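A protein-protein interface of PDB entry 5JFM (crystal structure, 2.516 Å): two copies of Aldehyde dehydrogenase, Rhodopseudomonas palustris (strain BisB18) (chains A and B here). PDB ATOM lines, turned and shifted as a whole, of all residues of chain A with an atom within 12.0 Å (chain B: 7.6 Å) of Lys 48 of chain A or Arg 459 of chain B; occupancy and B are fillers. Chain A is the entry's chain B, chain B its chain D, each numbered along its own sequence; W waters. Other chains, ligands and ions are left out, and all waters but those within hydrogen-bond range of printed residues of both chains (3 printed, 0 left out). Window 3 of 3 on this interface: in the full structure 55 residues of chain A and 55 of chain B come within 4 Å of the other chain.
OG1 of Thr 456 of chain B lies within hydrogen-bond range of O of Thr 308 of chain B (2.8 Å). The side-chain carboxylate (OD2) of Asp 457 of chain B lies within salt-bridge range of the guanidinium group (NH2) of Arg 459 of chain B, at 3.2 Å. The side-chain carboxylate (OD1) of Asp 306 of chain B sits at hydrogen-bond distance from the side-chain hydroxyl (OG1) of Thr 308 of chain B. The side-chain hydroxyl of Thr 308 of chain B sits at hydrogen-bond distance from the side-chain hydroxyl of Ser 455 of chain B. OG of Ser 455 of chain B sits at hydrogen-bond distance from N of Asp 457 of chain B (3.3 Å). The side-chain hydroxyl of Ser 51 of chain A is in hydrogen-bond range of the side-chain hydroxyl of Ser 49 of chain A, 2.9 Å away.
Among the printed residues, merely in contact across the chains: Lys 48 of chain A with Thr 308 of chain B (3.4 Å).
No position is printed for both chains. Of the 6 pairs that touch across the chains among the printed residues, none has its exchanged pair printed and touching as well.
Water W2 lies within hydrogen-bond range of O of Ser 52 of chain A (2.6 Å), NZ of Lys 463 of chain B (3.1 Å) and N of Ala 53 of chain A (3.4 Å). Water W3 bridges the side-chain carboxylate of Asp 457 of chain B (2.7 Å) and the side-chain amino group of Lys 48 of chain A (2.9 Å). Water W1 bridges the side-chain amide nitrogen (ND2) of Asn 50 of chain A and the guanidinium group (NH1) of Arg 459 of chain B.
Of the printed residues of chain B, Ser 49 of chain A touches Arg 459. Of the printed residues of chain B, Asn 50 of chain A touches Arg 459 (3.5 Å). Of the printed residues of chain B, Ser 52 of chain A touches Lys 460 (2.7 Å). No residue of chain A comes within 4 Å of Glu 307 of chain B. Printed residues of chain A within 4 Å of Asp 457 of chain B: Lys 48 (3.6 Å). No residue of chain A comes within 4 Å of Val 458 of chain B. Of the printed residues of chain A, Arg 459 of chain B touches Lys 48 (3.1 Å), Ser 49 (3.4 Å) and Asn 50 (3.5 Å). Printed residues of chain A within 4 Å of Lys 460 of chain B: Ser 52. No residue of chain A comes within 4 Å of Leu 461 of chain B. No residue of chain A comes within 4 Å of Thr 462 of chain B. The nearest printed residue of chain B that does not touch Asn 50 of chain A is Lys 460 of chain B (4.5 Å).
Of the 16 printed residues of chain A, 4 touch a printed residue of chain B. Along chain A the printed residues that touch a printed residue of chain B span positions 48 to 52. Of the 16 printed residues of chain B, 4 touch a printed residue of chain A. Among the printed residues, 6 pairs touch across the chains. Among the printed residues, Asp or Glu carboxylates within 4 Å of a Lys or Arg side-chain nitrogen of the other chain: Lys 48 of chain A with Asp 457 of chain B.
The backbone carbonyl oxygen of Ser 49 of chain A lies within hydrogen-bond range of the guanidinium group of Arg 459 of chain B, at 3.4 Å. OD1 of Asn 50 of chain A lies close to NH1 of Arg 459 of chain B. NZ of Lys 48 of chain A is in salt-bridge range of OD2 of Asp 457 of chain B. The backbone carbonyl oxygen of Lys 48 of chain A lies within hydrogen-bond range of the guanidinium group of Arg 459 of chain B. The side-chain hydroxyl of Ser 52 of chain A is in hydrogen-bond range of the side-chain amino group of Lys 460 of chain B.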
ATOM      1  N   LYS A  43      18.648 -27.580 -36.127  1.00  0.00           N
ATOM      2  CA  LYS A  43      17.773 -26.411 -36.040  1.00  0.00           C
ATOM      3  C   LYS A  43      16.962 -26.189 -37.321  1.00  0.00           C
ATOM      4  O   LYS A  43      17.432 -26.456 -38.433  1.00  0.00           O
ATOM      5  CB  LYS A  43      18.592 -25.163 -35.705  1.00  0.00           C
ATOM      6  CG  LYS A  43      19.193 -25.211 -34.309  1.00  0.00           C
ATOM      7  CD  LYS A  43      19.798 -23.875 -33.902  1.00  0.00           C
ATOM      8  CE  LYS A  43      20.777 -23.351 -34.955  1.00  0.00           C
ATOM      9  NZ  LYS A  43      21.722 -22.321 -34.398  1.00  0.00           N
ATOM     10  N   SER A  44      15.742 -25.692 -37.157  1.00  0.00           N
ATOM     11  CA  SER A  44      14.793 -25.668 -38.270  1.00  0.00           C
ATOM     12  C   SER A  44      15.014 -24.433 -39.136  1.00  0.00           C
ATOM     13  O   SER A  44      15.029 -23.313 -38.617  1.00  0.00           O
ATOM     14  CB  SER A  44      13.359 -25.691 -37.756  1.00  0.00           C
ATOM     15  OG  SER A  44      12.446 -25.644 -38.838  1.00  0.00           O
ATOM     16  N   PRO A  45      15.179 -24.591 -40.451  1.00  0.00           N
ATOM     17  CA  PRO A  45      15.380 -23.419 -41.320  1.00  0.00           C
ATOM     18  C   PRO A  45      14.109 -22.643 -41.638  1.00  0.00           C
ATOM     19  O   PRO A  45      14.199 -21.560 -42.238  1.00  0.00           O
ATOM     20  CB  PRO A  45      15.973 -24.034 -42.595  1.00  0.00           C
ATOM     21  CG  PRO A  45      15.402 -25.429 -42.623  1.00  0.00           C
ATOM     22  CD  PRO A  45      15.372 -25.864 -41.172  1.00  0.00           C
ATOM     23  N   ASP A  46      12.934 -23.155 -41.279  1.00  0.00           N
ATOM     24  CA  ASP A  46      11.696 -22.412 -41.493  1.00  0.00           C
ATOM     25  C   ASP A  46      10.939 -22.195 -40.183  1.00  0.00           C
ATOM     26  O   ASP A  46       9.715 -22.038 -40.178  1.00  0.00           O
ATOM     27  CB  ASP A  46      10.817 -23.088 -42.557  1.00  0.00           C
ATOM     28  CG  ASP A  46      10.473 -24.544 -42.233  1.00  0.00           C
ATOM     29  OD1 ASP A  46      11.024 -25.111 -41.261  1.00  0.00           O
ATOM     30  OD2 ASP A  46       9.660 -25.131 -42.985  1.00  0.00           O
ATOM     31  N   GLY A  47      11.671 -22.147 -39.068  1.00  0.00           N
ATOM     32  CA  GLY A  47      11.050 -21.912 -37.776  1.00  0.00           C
ATOM     33  C   GLY A  47      10.222 -23.100 -37.303  1.00  0.00           C
ATOM     34  O   GLY A  47      10.490 -24.261 -37.636  1.00  0.00           O
ATOM     35  N   LYS A  48       9.201 -22.797 -36.497  1.00  0.00           N
ATOM     36  CA  LYS A  48       8.277 -23.802 -35.972  1.00  0.00           C
ATOM     37  C   LYS A  48       6.862 -23.277 -36.184  1.00  0.00           C
ATOM     38  O   LYS A  48       6.342 -22.549 -35.336  1.00  0.00           O
ATOM     39  CB  LYS A  48       8.549 -24.084 -34.498  1.00  0.00           C
ATOM     40  CG  LYS A  48      10.015 -23.923 -34.091  1.00  0.00           C
ATOM     41  CD  LYS A  48      10.455 -24.980 -33.089  1.00  0.00           C
ATOM     42  CE  LYS A  48       9.391 -25.202 -32.028  1.00  0.00           C
ATOM     43  NZ  LYS A  48       9.866 -26.169 -31.011  1.00  0.00           N
ATOM     44  N   SER A  49       6.245 -23.631 -37.311  1.00  0.00           N
ATOM     45  CA  SER A  49       4.870 -23.229 -37.576  1.00  0.00           C
ATOM     46  C   SER A  49       3.940 -23.794 -36.502  1.00  0.00           C
ATOM     47  O   SER A  49       4.336 -24.611 -35.656  1.00  0.00           O
ATOM     48  CB  SER A  49       4.435 -23.697 -38.969  1.00  0.00           C
ATOM     49  OG  SER A  49       4.560 -25.107 -39.101  1.00  0.00           O
ATOM     50  N   ASN A  50       2.691 -23.344 -36.508  1.00  0.00           N
ATOM     51  CA  ASN A  50       1.725 -23.944 -35.588  1.00  0.00           C
ATOM     52  C   ASN A  50       0.726 -24.812 -36.336  1.00  0.00           C
ATOM     53  O   ASN A  50      -0.486 -24.572 -36.363  1.00  0.00           O
ATOM     54  CB  ASN A  50       1.056 -22.877 -34.728  1.00  0.00           C
ATOM     55  CG  ASN A  50       1.028 -23.275 -33.247  1.00  0.00           C
ATOM     56  OD1 ASN A  50       1.451 -24.387 -32.896  1.00  0.00           O
ATOM     57  ND2 ASN A  50       0.585 -22.366 -32.369  1.00  0.00           N
ATOM     58  N   SER A  51       1.278 -25.878 -36.934  1.00  0.00           N
ATOM     59  CA  SER A  51       0.503 -26.839 -37.703  1.00  0.00           C
ATOM     60  C   SER A  51      -0.503 -27.586 -36.830  1.00  0.00           C
ATOM     61  O   SER A  51      -1.542 -28.032 -37.334  1.00  0.00           O
ATOM     62  CB  SER A  51       1.452 -27.826 -38.386  1.00  0.00           C
ATOM     63  OG  SER A  51       2.443 -27.137 -39.136  1.00  0.00           O
ATOM     64  N   SER A  52      -0.225 -27.723 -35.530  1.00  0.00           N
ATOM     65  CA  SER A  52      -1.125 -28.397 -34.599  1.00  0.00           C
ATOM     66  C   SER A  52      -1.997 -27.437 -33.790  1.00  0.00           C
ATOM     67  O   SER A  52      -2.842 -27.899 -33.013  1.00  0.00           O
ATOM     68  CB  SER A  52      -0.333 -29.298 -33.642  1.00  0.00           C
ATOM     69  OG  SER A  52       0.577 -28.544 -32.863  1.00  0.00           O
ATOM     70  N   ALA A  53      -1.807 -26.118 -33.934  1.00  0.00           N
ATOM     71  CA  ALA A  53      -2.744 -25.167 -33.338  1.00  0.00           C
ATOM     72  C   ALA A  53      -4.067 -25.144 -34.083  1.00  0.00           C
ATOM     73  O   ALA A  53      -5.101 -24.794 -33.500  1.00  0.00           O
ATOM     74  CB  ALA A  53      -2.161 -23.758 -33.323  1.00  0.00           C
ATOM     75  N   ASP A  54      -4.051 -25.480 -35.368  1.00  0.00           N
ATOM     76  CA  ASP A  54      -5.277 -25.607 -36.128  1.00  0.00           C
ATOM     77  C   ASP A  54      -5.306 -26.956 -36.821  1.00  0.00           C
ATOM     78  O   ASP A  54      -5.459 -27.983 -36.164  1.00  0.00           O
ATOM     79  CB  ASP A  54      -5.412 -24.480 -37.142  1.00  0.00           C
ATOM     80  CG  ASP A  54      -6.853 -24.202 -37.493  1.00  0.00           C
ATOM     81  OD1 ASP A  54      -7.723 -24.509 -36.646  1.00  0.00           O
ATOM     82  OD2 ASP A  54      -7.114 -23.684 -38.601  1.00  0.00           O
ATOM     83  N   CYS A 515       0.913 -22.213 -11.196  1.00  0.00           N
ATOM     84  CA  CYS A 515       1.702 -22.627 -12.350  1.00  0.00           C
ATOM     85  C   CYS A 515       3.126 -22.133 -12.136  1.00  0.00           C
ATOM     86  O   CYS A 515       3.350 -20.927 -11.973  1.00  0.00           O
ATOM     87  CB  CYS A 515       1.096 -22.061 -13.635  1.00  0.00           C
ATOM     88  SG  CYS A 515       1.711 -22.739 -15.186  1.00  0.00           S
ATOM     89  N   MET A 517       6.893 -21.844 -13.385  1.00  0.00           N
ATOM     90  CA  MET A 517       7.898 -21.867 -14.448  1.00  0.00           C
ATOM     91  C   MET A 517       9.266 -21.847 -13.776  1.00  0.00           C
ATOM     92  O   MET A 517       9.729 -20.800 -13.311  1.00  0.00           O
ATOM     93  CB  MET A 517       7.715 -20.687 -15.399  1.00  0.00           C
ATOM     94  CG  MET A 517       8.747 -20.605 -16.527  1.00  0.00           C
ATOM     95  SD  MET A 517       8.442 -21.735 -17.918  1.00  0.00           S
ATOM     96  CE  MET A 517       6.829 -21.174 -18.463  1.00  0.00           C
ATOM     97  N   ALA A 520      12.793 -19.869 -15.458  1.00  0.00           N
ATOM     98  CA  ALA A 520      12.573 -19.063 -16.651  1.00  0.00           C
ATOM     99  C   ALA A 520      11.544 -17.992 -16.320  1.00  0.00           C
ATOM    100  O   ALA A 520      10.826 -18.079 -15.318  1.00  0.00           O
ATOM    101  CB  ALA A 520      12.105 -19.905 -17.843  1.00  0.00           C
ATOM    102  N   LEU A 521      11.492 -16.969 -17.169  1.00  0.00           N
ATOM    103  CA  LEU A 521      10.549 -15.858 -17.026  1.00  0.00           C
ATOM    104  C   LEU A 521      10.729 -15.085 -15.726  1.00  0.00           C
ATOM    105  O   LEU A 521       9.781 -14.468 -15.240  1.00  0.00           O
ATOM    106  CB  LEU A 521       9.104 -16.337 -17.156  1.00  0.00           C
ATOM    107  CG  LEU A 521       8.794 -16.673 -18.608  1.00  0.00           C
ATOM    108  CD1 LEU A 521       7.723 -17.716 -18.643  1.00  0.00           C
ATOM    109  CD2 LEU A 521       8.353 -15.409 -19.319  1.00  0.00           C
ATOM    110  N   ASP B 306       8.751 -33.491 -24.010  1.00  0.00           N
ATOM    111  CA  ASP B 306       8.692 -33.407 -25.462  1.00  0.00           C
ATOM    112  C   ASP B 306      10.088 -33.190 -26.037  1.00  0.00           C
ATOM    113  O   ASP B 306      11.086 -33.077 -25.311  1.00  0.00           O
ATOM    114  CB  ASP B 306       7.696 -32.326 -25.924  1.00  0.00           C
ATOM    115  CG  ASP B 306       8.178 -30.899 -25.682  1.00  0.00           C
ATOM    116  OD1 ASP B 306       9.319 -30.689 -25.230  1.00  0.00           O
ATOM    117  OD2 ASP B 306       7.400 -29.965 -25.988  1.00  0.00           O
ATOM    118  N   GLU B 307      10.148 -33.135 -27.366  1.00  0.00           N
ATOM    119  CA  GLU B 307      11.427 -33.120 -28.062  1.00  0.00           C
ATOM    120  C   GLU B 307      12.178 -31.803 -27.897  1.00  0.00           C
ATOM    121  O   GLU B 307      13.326 -31.714 -28.344  1.00  0.00           O
ATOM    122  CB  GLU B 307      11.202 -33.437 -29.542  1.00  0.00           C
ATOM    123  CG  GLU B 307      10.569 -32.322 -30.358  1.00  0.00           C
ATOM    124  CD  GLU B 307       9.077 -32.181 -30.124  1.00  0.00           C
ATOM    125  OE1 GLU B 307       8.532 -32.928 -29.281  1.00  0.00           O
ATOM    126  OE2 GLU B 307       8.456 -31.307 -30.777  1.00  0.00           O
ATOM    127  N   THR B 308      11.577 -30.792 -27.255  1.00  0.00           N
ATOM    128  CA  THR B 308      12.214 -29.497 -27.049  1.00  0.00           C
ATOM    129  C   THR B 308      12.855 -29.361 -25.673  1.00  0.00           C
ATOM    130  O   THR B 308      13.450 -28.323 -25.377  1.00  0.00           O
ATOM    131  CB  THR B 308      11.200 -28.359 -27.235  1.00  0.00           C
ATOM    132  OG1 THR B 308      10.233 -28.398 -26.171  1.00  0.00           O
ATOM    133  CG2 THR B 308      10.493 -28.459 -28.584  1.00  0.00           C
ATOM    134  N   ILE B 437       0.114 -34.582 -24.510  1.00  0.00           N
ATOM    135  CA  ILE B 437      -0.769 -33.732 -23.709  1.00  0.00           C
ATOM    136  C   ILE B 437      -2.121 -34.406 -23.496  1.00  0.00           C
ATOM    137  O   ILE B 437      -2.615 -34.486 -22.361  1.00  0.00           O
ATOM    138  CB  ILE B 437      -0.919 -32.341 -24.350  1.00  0.00           C
ATOM    139  CG1 ILE B 437       0.390 -31.561 -24.231  1.00  0.00           C
ATOM    140  CG2 ILE B 437      -2.035 -31.566 -23.684  1.00  0.00           C
ATOM    141  CD1 ILE B 437       0.402 -30.275 -25.020  1.00  0.00           C
ATOM    142  N   MET B 453       5.488 -30.781 -16.798  1.00  0.00           N
ATOM    143  CA  MET B 453       5.891 -30.819 -18.198  1.00  0.00           C
ATOM    144  C   MET B 453       7.320 -30.324 -18.351  1.00  0.00           C
ATOM    145  O   MET B 453       7.679 -29.273 -17.809  1.00  0.00           O
ATOM    146  CB  MET B 453       4.968 -29.970 -19.075  1.00  0.00           C
ATOM    147  CG  MET B 453       5.284 -30.064 -20.576  1.00  0.00           C
ATOM    148  SD  MET B 453       4.211 -29.021 -21.604  1.00  0.00           S
ATOM    149  CE  MET B 453       4.111 -30.008 -23.094  1.00  0.00           C
ATOM    150  N   SER B 455       9.551 -29.026 -21.321  1.00  0.00           N
ATOM    151  CA  SER B 455       9.415 -28.472 -22.660  1.00  0.00           C
ATOM    152  C   SER B 455       9.928 -27.038 -22.606  1.00  0.00           C
ATOM    153  O   SER B 455       9.726 -26.353 -21.600  1.00  0.00           O
ATOM    154  CB  SER B 455       7.942 -28.519 -23.119  1.00  0.00           C
ATOM    155  OG  SER B 455       7.736 -27.900 -24.378  1.00  0.00           O
ATOM    156  N   THR B 456      10.614 -26.597 -23.662  1.00  0.00           N
ATOM    157  CA  THR B 456      11.043 -25.202 -23.766  1.00  0.00           C
ATOM    158  C   THR B 456      10.143 -24.387 -24.681  1.00  0.00           C
ATOM    159  O   THR B 456      10.376 -23.186 -24.848  1.00  0.00           O
ATOM    160  CB  THR B 456      12.498 -25.100 -24.259  1.00  0.00           C
ATOM    161  OG1 THR B 456      12.611 -25.695 -25.557  1.00  0.00           O
ATOM    162  CG2 THR B 456      13.472 -25.778 -23.297  1.00  0.00           C
ATOM    163  N   ASP B 457       9.134 -25.019 -25.282  1.00  0.00           N
ATOM    164  CA  ASP B 457       8.185 -24.353 -26.165  1.00  0.00           C
ATOM    165  C   ASP B 457       7.099 -23.660 -25.337  1.00  0.00           C
ATOM    166  O   ASP B 457       6.306 -24.328 -24.654  1.00  0.00           O
ATOM    167  CB  ASP B 457       7.582 -25.387 -27.115  1.00  0.00           C
ATOM    168  CG  ASP B 457       6.835 -24.761 -28.272  1.00  0.00           C
ATOM    169  OD1 ASP B 457       6.335 -23.623 -28.131  1.00  0.00           O
ATOM    170  OD2 ASP B 457       6.736 -25.422 -29.324  1.00  0.00           O
ATOM    171  N   VAL B 458       7.055 -22.326 -25.400  1.00  0.00           N
ATOM    172  CA  VAL B 458       6.098 -21.581 -24.579  1.00  0.00           C
ATOM    173  C   VAL B 458       4.664 -21.871 -25.017  1.00  0.00           C
ATOM    174  O   VAL B 458       3.730 -21.799 -24.204  1.00  0.00           O
ATOM    175  CB  VAL B 458       6.414 -20.075 -24.621  1.00  0.00           C
ATOM    176  CG1 VAL B 458       6.084 -19.487 -25.978  1.00  0.00           C
ATOM    177  CG2 VAL B 458       5.659 -19.346 -23.548  1.00  0.00           C
ATOM    178  N   ARG B 459       4.460 -22.228 -26.290  1.00  0.00           N
ATOM    179  CA  ARG B 459       3.119 -22.576 -26.742  1.00  0.00           C
ATOM    180  C   ARG B 459       2.674 -23.913 -26.165  1.00  0.00           C
ATOM    181  O   ARG B 459       1.512 -24.073 -25.773  1.00  0.00           O
ATOM    182  CB  ARG B 459       3.072 -22.613 -28.265  1.00  0.00           C
ATOM    183  CG  ARG B 459       3.363 -21.272 -28.939  1.00  0.00           C
ATOM    184  CD  ARG B 459       3.588 -21.468 -30.430  1.00  0.00           C
ATOM    185  NE  ARG B 459       4.670 -22.421 -30.653  1.00  0.00           N
ATOM    186  CZ  ARG B 459       5.025 -22.896 -31.840  1.00  0.00           C
ATOM    187  NH1 ARG B 459       4.378 -22.507 -32.936  1.00  0.00           N
ATOM    188  NH2 ARG B 459       6.028 -23.761 -31.928  1.00  0.00           N
ATOM    189  N   LYS B 460       3.574 -24.895 -26.118  1.00  0.00           N
ATOM    190  CA  LYS B 460       3.177 -26.203 -25.621  1.00  0.00           C
ATOM    191  C   LYS B 460       3.062 -26.218 -24.101  1.00  0.00           C
ATOM    192  O   LYS B 460       2.204 -26.926 -23.555  1.00  0.00           O
ATOM    193  CB  LYS B 460       4.164 -27.270 -26.100  1.00  0.00           C
ATOM    194  CG  LYS B 460       4.309 -27.335 -27.605  1.00  0.00           C
ATOM    195  CD  LYS B 460       3.005 -27.718 -28.284  1.00  0.00           C
ATOM    196  CE  LYS B 460       3.156 -27.687 -29.822  1.00  0.00           C
ATOM    197  NZ  LYS B 460       1.923 -28.147 -30.556  1.00  0.00           N
ATOM    198  N   LEU B 461       3.915 -25.461 -23.403  1.00  0.00           N
ATOM    199  CA  LEU B 461       3.752 -25.304 -21.961  1.00  0.00           C
ATOM    200  C   LEU B 461       2.418 -24.639 -21.632  1.00  0.00           C
ATOM    201  O   LEU B 461       1.733 -25.038 -20.680  1.00  0.00           O
ATOM    202  CB  LEU B 461       4.910 -24.497 -21.385  1.00  0.00           C
ATOM    203  CG  LEU B 461       6.308 -25.110 -21.483  1.00  0.00           C
ATOM    204  CD1 LEU B 461       7.360 -24.030 -21.280  1.00  0.00           C
ATOM    205  CD2 LEU B 461       6.479 -26.227 -20.461  1.00  0.00           C
ATOM    206  N   THR B 462       2.024 -23.634 -22.419  1.00  0.00           N
ATOM    207  CA  THR B 462       0.737 -22.989 -22.191  1.00  0.00           C
ATOM    208  C   THR B 462      -0.408 -23.959 -22.438  1.00  0.00           C
ATOM    209  O   THR B 462      -1.313 -24.092 -21.603  1.00  0.00           O
ATOM    210  CB  THR B 462       0.596 -21.754 -23.079  1.00  0.00           C
ATOM    211  OG1 THR B 462       1.592 -20.795 -22.716  1.00  0.00           O
ATOM    212  CG2 THR B 462      -0.765 -21.120 -22.893  1.00  0.00           C
ATOM    213  N   LYS B 463      -0.372 -24.662 -23.573  1.00  0.00           N
ATOM    214  CA  LYS B 463      -1.468 -25.553 -23.935  1.00  0.00           C
ATOM    215  C   LYS B 463      -1.694 -26.614 -22.868  1.00  0.00           C
ATOM    216  O   LYS B 463      -2.829 -26.834 -22.431  1.00  0.00           O
ATOM    217  CB  LYS B 463      -1.199 -26.208 -25.285  1.00  0.00           C
ATOM    218  CG  LYS B 463      -2.296 -27.174 -25.695  1.00  0.00           C
ATOM    219  CD  LYS B 463      -1.979 -27.841 -27.009  1.00  0.00           C
ATOM    220  CE  LYS B 463      -3.161 -28.660 -27.521  1.00  0.00           C
ATOM    221  NZ  LYS B 463      -2.796 -29.392 -28.766  1.00  0.00           N
ATOM    222  N   MET B 464      -0.625 -27.282 -22.429  1.00  0.00           N
ATOM    223  CA  MET B 464      -0.823 -28.341 -21.449  1.00  0.00           C
ATOM    224  C   MET B 464      -1.296 -27.766 -20.123  1.00  0.00           C
ATOM    225  O   MET B 464      -2.201 -28.324 -19.487  1.00  0.00           O
ATOM    226  CB  MET B 464       0.450 -29.162 -21.261  1.00  0.00           C
ATOM    227  CG  MET B 464       0.227 -30.365 -20.333  1.00  0.00           C
ATOM    228  SD  MET B 464       1.684 -31.403 -20.060  1.00  0.00           S
ATOM    229  CE  MET B 464       1.107 -32.427 -18.702  1.00  0.00           C
ATOM    230  N   ALA B 465      -0.728 -26.632 -19.705  1.00  0.00           N
ATOM    231  CA  ALA B 465      -1.121 -26.055 -18.426  1.00  0.00           C
ATOM    232  C   ALA B 465      -2.578 -25.619 -18.463  1.00  0.00           C
ATOM    233  O   ALA B 465      -3.362 -25.946 -17.564  1.00  0.00           O
ATOM    234  CB  ALA B 465      -0.202 -24.886 -18.065  1.00  0.00           C
HETATM  235  O   HOH W   1       2.463 -19.779 -32.895  1.00  0.00           O
HETATM  236  O   HOH W   2      -1.756 -27.203 -30.743  1.00  0.00           O
HETATM  237  O   HOH W   3       7.673 -27.780 -30.121  1.00  0.00           O
